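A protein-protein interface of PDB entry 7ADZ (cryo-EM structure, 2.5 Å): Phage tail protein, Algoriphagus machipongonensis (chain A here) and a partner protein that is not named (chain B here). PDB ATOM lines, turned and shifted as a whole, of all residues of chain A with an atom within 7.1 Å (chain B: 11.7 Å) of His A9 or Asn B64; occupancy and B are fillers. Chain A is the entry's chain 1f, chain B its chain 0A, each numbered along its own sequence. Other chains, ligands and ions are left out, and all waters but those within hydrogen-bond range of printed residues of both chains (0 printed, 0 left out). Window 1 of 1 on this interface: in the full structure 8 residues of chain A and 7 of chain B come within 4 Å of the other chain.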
ATOM      1  N   SER A   6     -24.568 -24.831 -32.730  1.00  0.00           N
ATOM      2  CA  SER A   6     -23.288 -25.339 -32.263  1.00  0.00           C
ATOM      3  C   SER A   6     -23.400 -25.773 -30.805  1.00  0.00           C
ATOM      4  O   SER A   6     -24.361 -25.448 -30.110  1.00  0.00           O
ATOM      5  CB  SER A   6     -22.197 -24.285 -32.437  1.00  0.00           C
ATOM      6  OG  SER A   6     -22.610 -23.042 -31.906  1.00  0.00           O
ATOM      7  N   LYS A   7     -22.398 -26.513 -30.342  1.00  0.00           N
ATOM      8  CA  LYS A   7     -22.490 -27.199 -29.061  1.00  0.00           C
ATOM      9  C   LYS A   7     -21.391 -26.820 -28.070  1.00  0.00           C
ATOM     10  O   LYS A   7     -21.080 -27.601 -27.171  1.00  0.00           O
ATOM     11  CB  LYS A   7     -22.498 -28.711 -29.287  1.00  0.00           C
ATOM     12  CG  LYS A   7     -21.276 -29.261 -29.997  1.00  0.00           C
ATOM     13  CD  LYS A   7     -21.336 -30.768 -30.038  1.00  0.00           C
ATOM     14  CE  LYS A   7     -20.077 -31.359 -30.620  1.00  0.00           C
ATOM     15  NZ  LYS A   7     -20.089 -32.840 -30.543  1.00  0.00           N
ATOM     16  N   PHE A   8     -20.805 -25.627 -28.185  1.00  0.00           N
ATOM     17  CA  PHE A   8     -19.765 -25.226 -27.243  1.00  0.00           C
ATOM     18  C   PHE A   8     -20.202 -24.160 -26.244  1.00  0.00           C
ATOM     19  O   PHE A   8     -19.377 -23.721 -25.441  1.00  0.00           O
ATOM     20  CB  PHE A   8     -18.498 -24.760 -27.983  1.00  0.00           C
ATOM     21  CG  PHE A   8     -18.741 -23.762 -29.083  1.00  0.00           C
ATOM     22  CD1 PHE A   8     -18.932 -22.417 -28.803  1.00  0.00           C
ATOM     23  CD2 PHE A   8     -18.721 -24.166 -30.405  1.00  0.00           C
ATOM     24  CE1 PHE A   8     -19.145 -21.510 -29.816  1.00  0.00           C
ATOM     25  CE2 PHE A   8     -18.920 -23.258 -31.423  1.00  0.00           C
ATOM     26  CZ  PHE A   8     -19.135 -21.931 -31.127  1.00  0.00           C
ATOM     27  N   HIS A   9     -21.425 -23.649 -26.327  1.00  0.00           N
ATOM     28  CA  HIS A   9     -21.912 -22.631 -25.393  1.00  0.00           C
ATOM     29  C   HIS A   9     -23.124 -23.224 -24.636  1.00  0.00           C
ATOM     30  O   HIS A   9     -24.151 -23.468 -25.224  1.00  0.00           O
ATOM     31  CB  HIS A   9     -22.235 -21.371 -26.206  1.00  0.00           C
ATOM     32  CG  HIS A   9     -22.527 -20.158 -25.383  1.00  0.00           C
ATOM     33  ND1 HIS A   9     -21.897 -19.892 -24.190  1.00  0.00           N
ATOM     34  CD2 HIS A   9     -23.365 -19.119 -25.600  1.00  0.00           C
ATOM     35  CE1 HIS A   9     -22.351 -18.758 -23.694  1.00  0.00           C
ATOM     36  NE2 HIS A   9     -23.238 -18.264 -24.534  1.00  0.00           N
ATOM     37  N   PHE A  10     -23.011 -23.404 -23.325  1.00  0.00           N
ATOM     38  CA  PHE A  10     -24.026 -24.099 -22.542  1.00  0.00           C
ATOM     39  C   PHE A  10     -23.839 -23.773 -21.066  1.00  0.00           C
ATOM     40  O   PHE A  10     -22.809 -23.235 -20.660  1.00  0.00           O
ATOM     41  CB  PHE A  10     -23.985 -25.622 -22.786  1.00  0.00           C
ATOM     42  CG  PHE A  10     -22.645 -26.276 -22.503  1.00  0.00           C
ATOM     43  CD1 PHE A  10     -21.645 -26.305 -23.466  1.00  0.00           C
ATOM     44  CD2 PHE A  10     -22.406 -26.902 -21.285  1.00  0.00           C
ATOM     45  CE1 PHE A  10     -20.429 -26.908 -23.209  1.00  0.00           C
ATOM     46  CE2 PHE A  10     -21.194 -27.511 -21.026  1.00  0.00           C
ATOM     47  CZ  PHE A  10     -20.204 -27.515 -21.990  1.00  0.00           C
ATOM     48  N   SER A  11     -24.854 -24.104 -20.267  1.00  0.00           N
ATOM     49  CA  SER A  11     -24.826 -23.872 -18.828  1.00  0.00           C
ATOM     50  C   SER A  11     -25.580 -24.984 -18.110  1.00  0.00           C
ATOM     51  O   SER A  11     -26.431 -25.656 -18.692  1.00  0.00           O
ATOM     52  CB  SER A  11     -25.421 -22.506 -18.463  1.00  0.00           C
ATOM     53  OG  SER A  11     -26.792 -22.426 -18.790  1.00  0.00           O
ATOM     54  N   ILE A  19     -21.572 -22.462 -12.701  1.00  0.00           N
ATOM     55  CA  ILE A  19     -22.364 -23.121 -13.734  1.00  0.00           C
ATOM     56  C   ILE A  19     -21.557 -23.464 -14.979  1.00  0.00           C
ATOM     57  O   ILE A  19     -22.124 -23.994 -15.941  1.00  0.00           O
ATOM     58  CB  ILE A  19     -23.588 -22.265 -14.131  1.00  0.00           C
ATOM     59  CG1 ILE A  19     -23.147 -20.989 -14.844  1.00  0.00           C
ATOM     60  CG2 ILE A  19     -24.440 -21.944 -12.918  1.00  0.00           C
ATOM     61  CD1 ILE A  19     -24.285 -20.153 -15.352  1.00  0.00           C
ATOM     62  N   GLY A  20     -20.251 -23.196 -14.990  1.00  0.00           N
ATOM     63  CA  GLY A  20     -19.431 -23.461 -16.160  1.00  0.00           C
ATOM     64  C   GLY A  20     -18.721 -24.799 -16.088  1.00  0.00           C
ATOM     65  O   GLY A  20     -17.988 -25.074 -15.137  1.00  0.00           O
ATOM     66  N   PHE A  21     -18.933 -25.625 -17.112  1.00  0.00           N
ATOM     67  CA  PHE A  21     -18.402 -26.979 -17.167  1.00  0.00           C
ATOM     68  C   PHE A  21     -17.632 -27.166 -18.468  1.00  0.00           C
ATOM     69  O   PHE A  21     -17.582 -26.268 -19.310  1.00  0.00           O
ATOM     70  CB  PHE A  21     -19.525 -28.024 -17.061  1.00  0.00           C
ATOM     71  CG  PHE A  21     -20.106 -28.166 -15.683  1.00  0.00           C
ATOM     72  CD1 PHE A  21     -21.014 -27.238 -15.194  1.00  0.00           C
ATOM     73  CD2 PHE A  21     -19.756 -29.240 -14.879  1.00  0.00           C
ATOM     74  CE1 PHE A  21     -21.549 -27.365 -13.930  1.00  0.00           C
ATOM     75  CE2 PHE A  21     -20.292 -29.377 -13.615  1.00  0.00           C
ATOM     76  CZ  PHE A  21     -21.189 -28.438 -13.141  1.00  0.00           C
ATOM     77  N   THR A  22     -17.018 -28.340 -18.632  1.00  0.00           N
ATOM     78  CA  THR A  22     -16.301 -28.635 -19.870  1.00  0.00           C
ATOM     79  C   THR A  22     -17.029 -29.610 -20.788  1.00  0.00           C
ATOM     80  O   THR A  22     -17.010 -29.405 -22.003  1.00  0.00           O
ATOM     81  CB  THR A  22     -14.888 -29.173 -19.586  1.00  0.00           C
ATOM     82  OG1 THR A  22     -14.952 -30.349 -18.774  1.00  0.00           O
ATOM     83  CG2 THR A  22     -14.033 -28.129 -18.901  1.00  0.00           C
ATOM     84  N   SER A  91     -29.006 -26.202 -20.368  1.00  0.00           N
ATOM     85  CA  SER A  91     -29.488 -25.378 -21.471  1.00  0.00           C
ATOM     86  C   SER A  91     -28.402 -25.172 -22.516  1.00  0.00           C
ATOM     87  O   SER A  91     -27.223 -25.063 -22.178  1.00  0.00           O
ATOM     88  CB  SER A  91     -29.973 -24.009 -20.978  1.00  0.00           C
ATOM     89  OG  SER A  91     -31.137 -24.123 -20.185  1.00  0.00           O
ATOM     90  N   LEU A  92     -28.812 -25.116 -23.780  1.00  0.00           N
ATOM     91  CA  LEU A  92     -27.953 -24.705 -24.883  1.00  0.00           C
ATOM     92  C   LEU A  92     -28.279 -23.261 -25.248  1.00  0.00           C
ATOM     93  O   LEU A  92     -29.448 -22.916 -25.433  1.00  0.00           O
ATOM     94  CB  LEU A  92     -28.162 -25.634 -26.080  1.00  0.00           C
ATOM     95  CG  LEU A  92     -27.257 -25.561 -27.308  1.00  0.00           C
ATOM     96  CD1 LEU A  92     -25.809 -25.735 -26.918  1.00  0.00           C
ATOM     97  CD2 LEU A  92     -27.655 -26.626 -28.300  1.00  0.00           C
ATOM     98  N   LEU A  93     -27.255 -22.417 -25.342  1.00  0.00           N
ATOM     99  CA  LEU A  93     -27.448 -20.974 -25.427  1.00  0.00           C
ATOM    100  C   LEU A  93     -27.139 -20.434 -26.820  1.00  0.00           C
ATOM    101  O   LEU A  93     -26.346 -21.009 -27.567  1.00  0.00           O
ATOM    102  CB  LEU A  93     -26.575 -20.255 -24.397  1.00  0.00           C
ATOM    103  CG  LEU A  93     -26.684 -20.746 -22.952  1.00  0.00           C
ATOM    104  CD1 LEU A  93     -25.537 -20.218 -22.118  1.00  0.00           C
ATOM    105  CD2 LEU A  93     -28.019 -20.353 -22.335  1.00  0.00           C
ATOM    106  N   ASN A  94     -27.777 -19.310 -27.161  1.00  0.00           N
ATOM    107  CA  ASN A  94     -27.494 -18.602 -28.405  1.00  0.00           C
ATOM    108  C   ASN A  94     -26.436 -17.520 -28.163  1.00  0.00           C
ATOM    109  O   ASN A  94     -25.751 -17.508 -27.139  1.00  0.00           O
ATOM    110  CB  ASN A  94     -28.782 -18.049 -29.033  1.00  0.00           C
ATOM    111  CG  ASN A  94     -29.608 -17.167 -28.091  1.00  0.00           C
ATOM    112  OD1 ASN A  94     -29.093 -16.481 -27.213  1.00  0.00           O
ATOM    113  ND2 ASN A  94     -30.918 -17.182 -28.296  1.00  0.00           N
ATOM    114  N   GLU A  95     -26.298 -16.595 -29.113  1.00  0.00           N
ATOM    115  CA  GLU A  95     -25.233 -15.596 -29.039  1.00  0.00           C
ATOM    116  C   GLU A  95     -25.515 -14.520 -27.996  1.00  0.00           C
ATOM    117  O   GLU A  95     -24.577 -13.922 -27.462  1.00  0.00           O
ATOM    118  CB  GLU A  95     -25.015 -14.964 -30.409  1.00  0.00           C
ATOM    119  CG  GLU A  95     -24.082 -15.755 -31.303  1.00  0.00           C
ATOM    120  CD  GLU A  95     -24.787 -16.865 -32.054  1.00  0.00           C
ATOM    121  OE1 GLU A  95     -24.091 -17.690 -32.679  1.00  0.00           O
ATOM    122  OE2 GLU A  95     -26.031 -16.916 -32.023  1.00  0.00           O
ATOM    123  N   GLU A  96     -26.785 -14.245 -27.706  1.00  0.00           N
ATOM    124  CA  GLU A  96     -27.123 -13.345 -26.610  1.00  0.00           C
ATOM    125  C   GLU A  96     -27.423 -14.078 -25.306  1.00  0.00           C
ATOM    126  O   GLU A  96     -28.125 -13.525 -24.454  1.00  0.00           O
ATOM    127  CB  GLU A  96     -28.289 -12.432 -27.010  1.00  0.00           C
ATOM    128  CG  GLU A  96     -29.572 -13.126 -27.421  1.00  0.00           C
ATOM    129  CD  GLU A  96     -29.647 -13.370 -28.921  1.00  0.00           C
ATOM    130  OE1 GLU A  96     -28.600 -13.276 -29.594  1.00  0.00           O
ATOM    131  OE2 GLU A  96     -30.753 -13.651 -29.430  1.00  0.00           O
ATOM    132  N   HIS A  97     -26.896 -15.296 -25.146  1.00  0.00           N
ATOM    133  CA  HIS A  97     -26.854 -16.080 -23.910  1.00  0.00           C
ATOM    134  C   HIS A  97     -28.232 -16.431 -23.356  1.00  0.00           C
ATOM    135  O   HIS A  97     -28.421 -16.440 -22.139  1.00  0.00           O
ATOM    136  CB  HIS A  97     -26.014 -15.380 -22.826  1.00  0.00           C
ATOM    137  CG  HIS A  97     -24.834 -14.629 -23.362  1.00  0.00           C
ATOM    138  ND1 HIS A  97     -23.730 -15.256 -23.896  1.00  0.00           N
ATOM    139  CD2 HIS A  97     -24.596 -13.301 -23.469  1.00  0.00           C
ATOM    140  CE1 HIS A  97     -22.862 -14.349 -24.304  1.00  0.00           C
ATOM    141  NE2 HIS A  97     -23.363 -13.154 -24.053  1.00  0.00           N
ATOM    142  N   GLU A  98     -29.196 -16.743 -24.214  1.00  0.00           N
ATOM    143  CA  GLU A  98     -30.532 -17.156 -23.813  1.00  0.00           C
ATOM    144  C   GLU A  98     -30.789 -18.612 -24.193  1.00  0.00           C
ATOM    145  O   GLU A  98     -30.212 -19.115 -25.163  1.00  0.00           O
ATOM    146  CB  GLU A  98     -31.585 -16.244 -24.462  1.00  0.00           C
ATOM    147  CG  GLU A  98     -31.453 -14.767 -24.093  1.00  0.00           C
ATOM    148  CD  GLU A  98     -32.211 -14.381 -22.829  1.00  0.00           C
ATOM    149  OE1 GLU A  98     -32.218 -15.155 -21.849  1.00  0.00           O
ATOM    150  OE2 GLU A  98     -32.803 -13.284 -22.816  1.00  0.00           O
ATOM    151  N   GLU B  58      -6.438 -21.083 -26.159  1.00  0.00           N
ATOM    152  CA  GLU B  58      -7.524 -20.578 -25.328  1.00  0.00           C
ATOM    153  C   GLU B  58      -7.756 -21.528 -24.160  1.00  0.00           C
ATOM    154  O   GLU B  58      -7.792 -22.748 -24.346  1.00  0.00           O
ATOM    155  CB  GLU B  58      -8.809 -20.419 -26.142  1.00  0.00           C
ATOM    156  CG  GLU B  58      -9.957 -19.796 -25.372  1.00  0.00           C
ATOM    157  CD  GLU B  58     -11.216 -19.685 -26.199  1.00  0.00           C
ATOM    158  OE1 GLU B  58     -11.198 -20.135 -27.363  1.00  0.00           O
ATOM    159  OE2 GLU B  58     -12.224 -19.151 -25.688  1.00  0.00           O
ATOM    160  N   GLU B  59      -7.900 -20.969 -22.960  1.00  0.00           N
ATOM    161  CA  GLU B  59      -8.193 -21.776 -21.783  1.00  0.00           C
ATOM    162  C   GLU B  59      -9.651 -22.224 -21.780  1.00  0.00           C
ATOM    163  O   GLU B  59     -10.568 -21.403 -21.819  1.00  0.00           O
ATOM    164  CB  GLU B  59      -7.871 -20.988 -20.512  1.00  0.00           C
ATOM    165  CG  GLU B  59      -8.226 -21.719 -19.224  1.00  0.00           C
ATOM    166  CD  GLU B  59      -7.407 -22.977 -19.002  1.00  0.00           C
ATOM    167  OE1 GLU B  59      -6.226 -23.014 -19.406  1.00  0.00           O
ATOM    168  OE2 GLU B  59      -7.958 -23.948 -18.445  1.00  0.00           O
ATOM    169  N   VAL B  60      -9.857 -23.542 -21.700  1.00  0.00           N
ATOM    170  CA  VAL B  60     -11.174 -24.142 -21.898  1.00  0.00           C
ATOM    171  C   VAL B  60     -11.995 -24.214 -20.617  1.00  0.00           C
ATOM    172  O   VAL B  60     -13.227 -24.075 -20.676  1.00  0.00           O
ATOM    173  CB  VAL B  60     -10.988 -25.541 -22.524  1.00  0.00           C
ATOM    174  CG1 VAL B  60     -12.319 -26.194 -22.900  1.00  0.00           C
ATOM    175  CG2 VAL B  60     -10.092 -25.447 -23.737  1.00  0.00           C
ATOM    176  N   THR B  61     -11.355 -24.358 -19.454  1.00  0.00           N
ATOM    177  CA  THR B  61     -12.079 -24.549 -18.200  1.00  0.00           C
ATOM    178  C   THR B  61     -12.847 -23.307 -17.757  1.00  0.00           C
ATOM    179  O   THR B  61     -13.765 -23.419 -16.941  1.00  0.00           O
ATOM    180  CB  THR B  61     -11.114 -24.974 -17.089  1.00  0.00           C
ATOM    181  OG1 THR B  61     -10.189 -23.918 -16.821  1.00  0.00           O
ATOM    182  CG2 THR B  61     -10.345 -26.216 -17.484  1.00  0.00           C
ATOM    183  N   MET B  62     -12.504 -22.129 -18.276  1.00  0.00           N
ATOM    184  CA  MET B  62     -13.149 -20.881 -17.889  1.00  0.00           C
ATOM    185  C   MET B  62     -14.025 -20.294 -18.988  1.00  0.00           C
ATOM    186  O   MET B  62     -14.390 -19.119 -18.909  1.00  0.00           O
ATOM    187  CB  MET B  62     -12.094 -19.857 -17.475  1.00  0.00           C
ATOM    188  CG  MET B  62     -11.009 -20.406 -16.574  1.00  0.00           C
ATOM    189  SD  MET B  62      -9.746 -19.176 -16.227  1.00  0.00           S
ATOM    190  CE  MET B  62     -10.565 -18.237 -14.948  1.00  0.00           C
ATOM    191  N   LYS B  63     -14.376 -21.084 -20.002  1.00  0.00           N
ATOM    192  CA  LYS B  63     -14.969 -20.525 -21.213  1.00  0.00           C
ATOM    193  C   LYS B  63     -16.440 -20.159 -21.019  1.00  0.00           C
ATOM    194  O   LYS B  63     -16.915 -19.161 -21.571  1.00  0.00           O
ATOM    195  CB  LYS B  63     -14.807 -21.519 -22.358  1.00  0.00           C
ATOM    196  CG  LYS B  63     -15.034 -20.940 -23.725  1.00  0.00           C
ATOM    197  CD  LYS B  63     -15.041 -22.023 -24.780  1.00  0.00           C
ATOM    198  CE  LYS B  63     -15.401 -21.454 -26.133  1.00  0.00           C
ATOM    199  NZ  LYS B  63     -15.531 -22.516 -27.157  1.00  0.00           N
ATOM    200  N   ASN B  64     -17.176 -20.947 -20.244  1.00  0.00           N
ATOM    201  CA  ASN B  64     -18.607 -20.750 -20.074  1.00  0.00           C
ATOM    202  C   ASN B  64     -18.963 -20.025 -18.782  1.00  0.00           C
ATOM    203  O   ASN B  64     -20.067 -20.214 -18.271  1.00  0.00           O
ATOM    204  CB  ASN B  64     -19.331 -22.099 -20.136  1.00  0.00           C
ATOM    205  CG  ASN B  64     -19.481 -22.613 -21.554  1.00  0.00           C
ATOM    206  OD1 ASN B  64     -20.060 -21.949 -22.405  1.00  0.00           O
ATOM    207  ND2 ASN B  64     -18.938 -23.790 -21.817  1.00  0.00           N
ATOM    208  N   PHE B  65     -18.058 -19.215 -18.240  1.00  0.00           N
ATOM    209  CA  PHE B  65     -18.353 -18.469 -17.022  1.00  0.00           C
ATOM    210  C   PHE B  65     -19.146 -17.206 -17.359  1.00  0.00           C
ATOM    211  O   PHE B  65     -18.854 -16.540 -18.354  1.00  0.00           O
ATOM    212  CB  PHE B  65     -17.065 -18.078 -16.291  1.00  0.00           C
ATOM    213  CG  PHE B  65     -16.396 -19.203 -15.531  1.00  0.00           C
ATOM    214  CD1 PHE B  65     -16.864 -20.510 -15.584  1.00  0.00           C
ATOM    215  CD2 PHE B  65     -15.278 -18.938 -14.759  1.00  0.00           C
ATOM    216  CE1 PHE B  65     -16.231 -21.519 -14.887  1.00  0.00           C
ATOM    217  CE2 PHE B  65     -14.645 -19.943 -14.054  1.00  0.00           C
ATOM    218  CZ  PHE B  65     -15.123 -21.235 -14.121  1.00  0.00           C
ATOM    219  N   PRO B  66     -20.145 -16.850 -16.554  1.00  0.00           N
ATOM    220  CA  PRO B  66     -20.904 -15.619 -16.804  1.00  0.00           C
ATOM    221  C   PRO B  66     -20.223 -14.385 -16.231  1.00  0.00           C
ATOM    222  O   PRO B  66     -19.253 -14.472 -15.477  1.00  0.00           O
ATOM    223  CB  PRO B  66     -22.244 -15.879 -16.099  1.00  0.00           C
ATOM    224  CG  PRO B  66     -22.189 -17.295 -15.607  1.00  0.00           C
ATOM    225  CD  PRO B  66     -20.756 -17.653 -15.488  1.00  0.00           C
ATOM    226  N   ASN B  67     -20.760 -13.212 -16.597  1.00  0.00           N
ATOM    227  CA  ASN B  67     -20.133 -11.933 -16.272  1.00  0.00           C
ATOM    228  C   ASN B  67     -21.148 -10.827 -15.966  1.00  0.00           C
ATOM    229  O   ASN B  67     -20.891  -9.662 -16.276  1.00  0.00           O
ATOM    230  CB  ASN B  67     -19.207 -11.506 -17.415  1.00  0.00           C
ATOM    231  CG  ASN B  67     -18.059 -10.634 -16.954  1.00  0.00           C
ATOM    232  OD1 ASN B  67     -17.716 -10.612 -15.775  1.00  0.00           O
ATOM    233  ND2 ASN B  67     -17.464  -9.902 -17.885  1.00  0.00           N
ATOM    234  N   ASN B  68     -22.296 -11.151 -15.378  1.00  0.00           N
ATOM    235  CA  ASN B  68     -23.289 -10.133 -15.053  1.00  0.00           C
ATOM    236  C   ASN B  68     -23.036  -9.530 -13.674  1.00  0.00           C
ATOM    237  O   ASN B  68     -22.392 -10.136 -12.816  1.00  0.00           O
ATOM    238  CB  ASN B  68     -24.693 -10.724 -15.114  1.00  0.00           C
ATOM    239  CG  ASN B  68     -25.004 -11.328 -16.459  1.00  0.00           C
ATOM    240  OD1 ASN B  68     -24.579 -10.817 -17.488  1.00  0.00           O
ATOM    241  ND2 ASN B  68     -25.745 -12.423 -16.458  1.00  0.00           N
ATOM    242  N   TYR B  77     -25.836  -6.347 -18.016  1.00  0.00           N
ATOM    243  CA  TYR B  77     -25.414  -7.533 -18.754  1.00  0.00           C
ATOM    244  C   TYR B  77     -24.126  -7.260 -19.522  1.00  0.00           C
ATOM    245  O   TYR B  77     -23.996  -6.214 -20.162  1.00  0.00           O
ATOM    246  CB  TYR B  77     -26.510  -7.970 -19.722  1.00  0.00           C
ATOM    247  CG  TYR B  77     -27.756  -8.503 -19.069  1.00  0.00           C
ATOM    248  CD1 TYR B  77     -27.843  -9.831 -18.683  1.00  0.00           C
ATOM    249  CD2 TYR B  77     -28.855  -7.682 -18.851  1.00  0.00           C
ATOM    250  CE1 TYR B  77     -28.979 -10.329 -18.091  1.00  0.00           C
ATOM    251  CE2 TYR B  77     -30.000  -8.170 -18.256  1.00  0.00           C
ATOM    252  CZ  TYR B  77     -30.055  -9.498 -17.880  1.00  0.00           C
ATOM    253  OH  TYR B  77     -31.187 -10.003 -17.289  1.00  0.00           O
ATOM    254  N   LYS B  78     -23.169  -8.191 -19.443  1.00  0.00           N
ATOM    255  CA  LYS B  78     -21.904  -8.106 -20.168  1.00  0.00           C
ATOM    256  C   LYS B  78     -21.569  -9.456 -20.796  1.00  0.00           C
ATOM    257  O   LYS B  78     -22.091 -10.495 -20.392  1.00  0.00           O
ATOM    258  CB  LYS B  78     -20.725  -7.682 -19.268  1.00  0.00           C
ATOM    259  CG  LYS B  78     -21.027  -6.659 -18.195  1.00  0.00           C
ATOM    260  CD  LYS B  78     -19.791  -5.912 -17.774  1.00  0.00           C
ATOM    261  CE  LYS B  78     -20.111  -4.927 -16.678  1.00  0.00           C
ATOM    262  NZ  LYS B  78     -19.079  -3.873 -16.558  1.00  0.00           N
ATOM    263  N   ASN B  79     -20.667  -9.430 -21.794  1.00  0.00           N
ATOM    264  CA  ASN B  79     -20.174 -10.639 -22.446  1.00  0.00           C
ATOM    265  C   ASN B  79     -19.101 -11.325 -21.596  1.00  0.00           C
ATOM    266  O   ASN B  79     -18.411 -10.666 -20.814  1.00  0.00           O
ATOM    267  CB  ASN B  79     -19.601 -10.310 -23.821  1.00  0.00           C
ATOM    268  CG  ASN B  79     -20.644  -9.797 -24.777  1.00  0.00           C
ATOM    269  OD1 ASN B  79     -21.588 -10.500 -25.118  1.00  0.00           O
ATOM    270  ND2 ASN B  79     -20.479  -8.561 -25.219  1.00  0.00           N
ATOM    271  N   PRO B  80     -18.956 -12.649 -21.714  1.00  0.00           N
ATOM    272  CA  PRO B  80     -17.901 -13.350 -20.967  1.00  0.00           C
ATOM    273  C   PRO B  80     -16.499 -13.005 -21.456  1.00  0.00           C
ATOM    274  O   PRO B  80     -16.275 -12.749 -22.639  1.00  0.00           O
ATOM    275  CB  PRO B  80     -18.221 -14.829 -21.205  1.00  0.00           C
ATOM    276  CG  PRO B  80     -19.642 -14.862 -21.598  1.00  0.00           C
ATOM    277  CD  PRO B  80     -19.901 -13.596 -22.334  1.00  0.00           C
ATOM    278  N   LYS B  81     -15.547 -13.034 -20.528  1.00  0.00           N
ATOM    279  CA  LYS B  81     -14.158 -12.693 -20.795  1.00  0.00           C
ATOM    280  C   LYS B  81     -13.440 -13.815 -21.542  1.00  0.00           C
ATOM    281  O   LYS B  81     -13.839 -14.980 -21.513  1.00  0.00           O
ATOM    282  CB  LYS B  81     -13.415 -12.396 -19.496  1.00  0.00           C
ATOM    283  CG  LYS B  81     -14.101 -11.402 -18.595  1.00  0.00           C
ATOM    284  CD  LYS B  81     -13.382 -11.280 -17.270  1.00  0.00           C
ATOM    285  CE  LYS B  81     -14.217 -10.503 -16.275  1.00  0.00           C
ATOM    286  NZ  LYS B  81     -13.465 -10.187 -15.039  1.00  0.00           N
ATOM    287  N   LEU B  82     -12.537 -13.626 -22.315  1.00  0.00           N
ATOM    288  CA  LEU B  82     -11.665 -14.399 -23.193  1.00  0.00           C
ATOM    289  C   LEU B  82     -10.404 -14.806 -22.430  1.00  0.00           C
ATOM    290  O   LEU B  82      -9.722 -13.957 -21.856  1.00  0.00           O
ATOM    291  CB  LEU B  82     -11.305 -13.522 -24.404  1.00  0.00           C
ATOM    292  CG  LEU B  82     -10.551 -14.012 -25.645  1.00  0.00           C
ATOM    293  CD1 LEU B  82     -10.713 -15.515 -25.813  1.00  0.00           C
ATOM    294  CD2 LEU B  82     -11.028 -13.275 -26.887  1.00  0.00           C
ATOM    295  N   ASN B  83      -9.810 -15.776 -22.163  1.00  0.00           N
ATOM    296  CA  ASN B  83      -8.546 -16.092 -21.498  1.00  0.00           C
ATOM    297  C   ASN B  83      -7.604 -16.836 -22.446  1.00  0.00           C
ATOM    298  O   ASN B  83      -8.012 -17.796 -23.104  1.00  0.00           O
ATOM    299  CB  ASN B  83      -8.799 -16.913 -20.233  1.00  0.00           C
ATOM    300  CG  ASN B  83      -9.868 -16.303 -19.338  1.00  0.00           C
ATOM    301  OD1 ASN B  83      -9.593 -15.404 -18.550  1.00  0.00           O
ATOM    302  ND2 ASN B  83     -11.090 -16.803 -19.446  1.00  0.00           N
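The backbone NH of Phe A10 lies within hydrogen-bond range of the side-chain amide oxygen of Asn B64 (3.4 Å). OD1 of Asn B79 is in hydrogen-bond range of NE2 of His A97 (3.4 Å). ND1 of His A9 sits at hydrogen-bond distance from OD1 of Asn B64 (3.3 Å).
The backbone NH of Leu A93 sits at hydrogen-bond distance from the backbone carbonyl oxygen of His A9 (3.3 Å). A ring nitrogen (ND1) of His A97 lies within hydrogen-bond range of a ring nitrogen (NE2) of His A9, at 3.1 Å. The side-chain amide nitrogen of Asn B67 is in hydrogen-bond range of the backbone carbonyl oxygen of Asn B79, at 3.2 Å. The backbone NH of His A97 sits at hydrogen-bond distance from the side-chain amide oxygen of Asn A94 (3.2 Å).
NZ of Lys B63 touches CD1 of Phe A8, 3.8 Å away. Phe A8 touches Asn B64. CG of Pro B66 touches CD1 of Ile A19 (3.6 Å). CA of Gly A20 touches O of Asn B64, 3.9 Å away. Phe B65 touches Gly A20 (CD1 to CA, 3.95 Å). Asn B64 touches Phe A21 (ND2 to O, 3.8 Å). His A97 touches Pro B80 (CE1 to CD, 3.6 Å).
No residue of chain B comes within 4 Å of Ser A6. Of the printed residues of chain B, His A9 touches Asn B64. Of chain B, only Asn B64 (3.4 Å) comes within 4 Å of Phe A10. No residue of chain B comes within 4 Å of Ser A11. Of chain B, only Asn B64 (3.9 Å) and Phe B65 (3.95 Å) come within 4 Å of Gly A20. No residue of chain B comes within 4 Å of Leu A92. No residue of chain B comes within 4 Å of Leu A93. No residue of chain B comes within 4 Å of Glu A95. Of chain B, only Asn B79 and Pro B80 come within 4 Å of His A97. Printed residues of chain A within 4 Å of Lys B63: Phe A8 (3.8 Å). Asn B64 touches just these residues of chain A: Phe A8, His A9, Phe A10, Gly A20 and Phe A21. Of the printed residues of chain A, Phe B65 touches Gly A20. Lys B78 touches none of the printed residues of chain A. Of the printed residues of chain A, Pro B80 touches His A97 (3.6 Å). The nearest printed residue of chain A that does not touch Pro B80 is His A9 (5.2 Å).
Hydrophobic or aromatic side chains of chain A that line the printed part of chain B: Phe A8, His A9, Phe A10, Ile A19 and His A97. Hydrophobic or aromatic side chains of chain B within 4 Å of the printed part of chain A: Phe B65, Pro B66 and Pro B80. Among the printed residues, 10 pairs touch across the chains.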
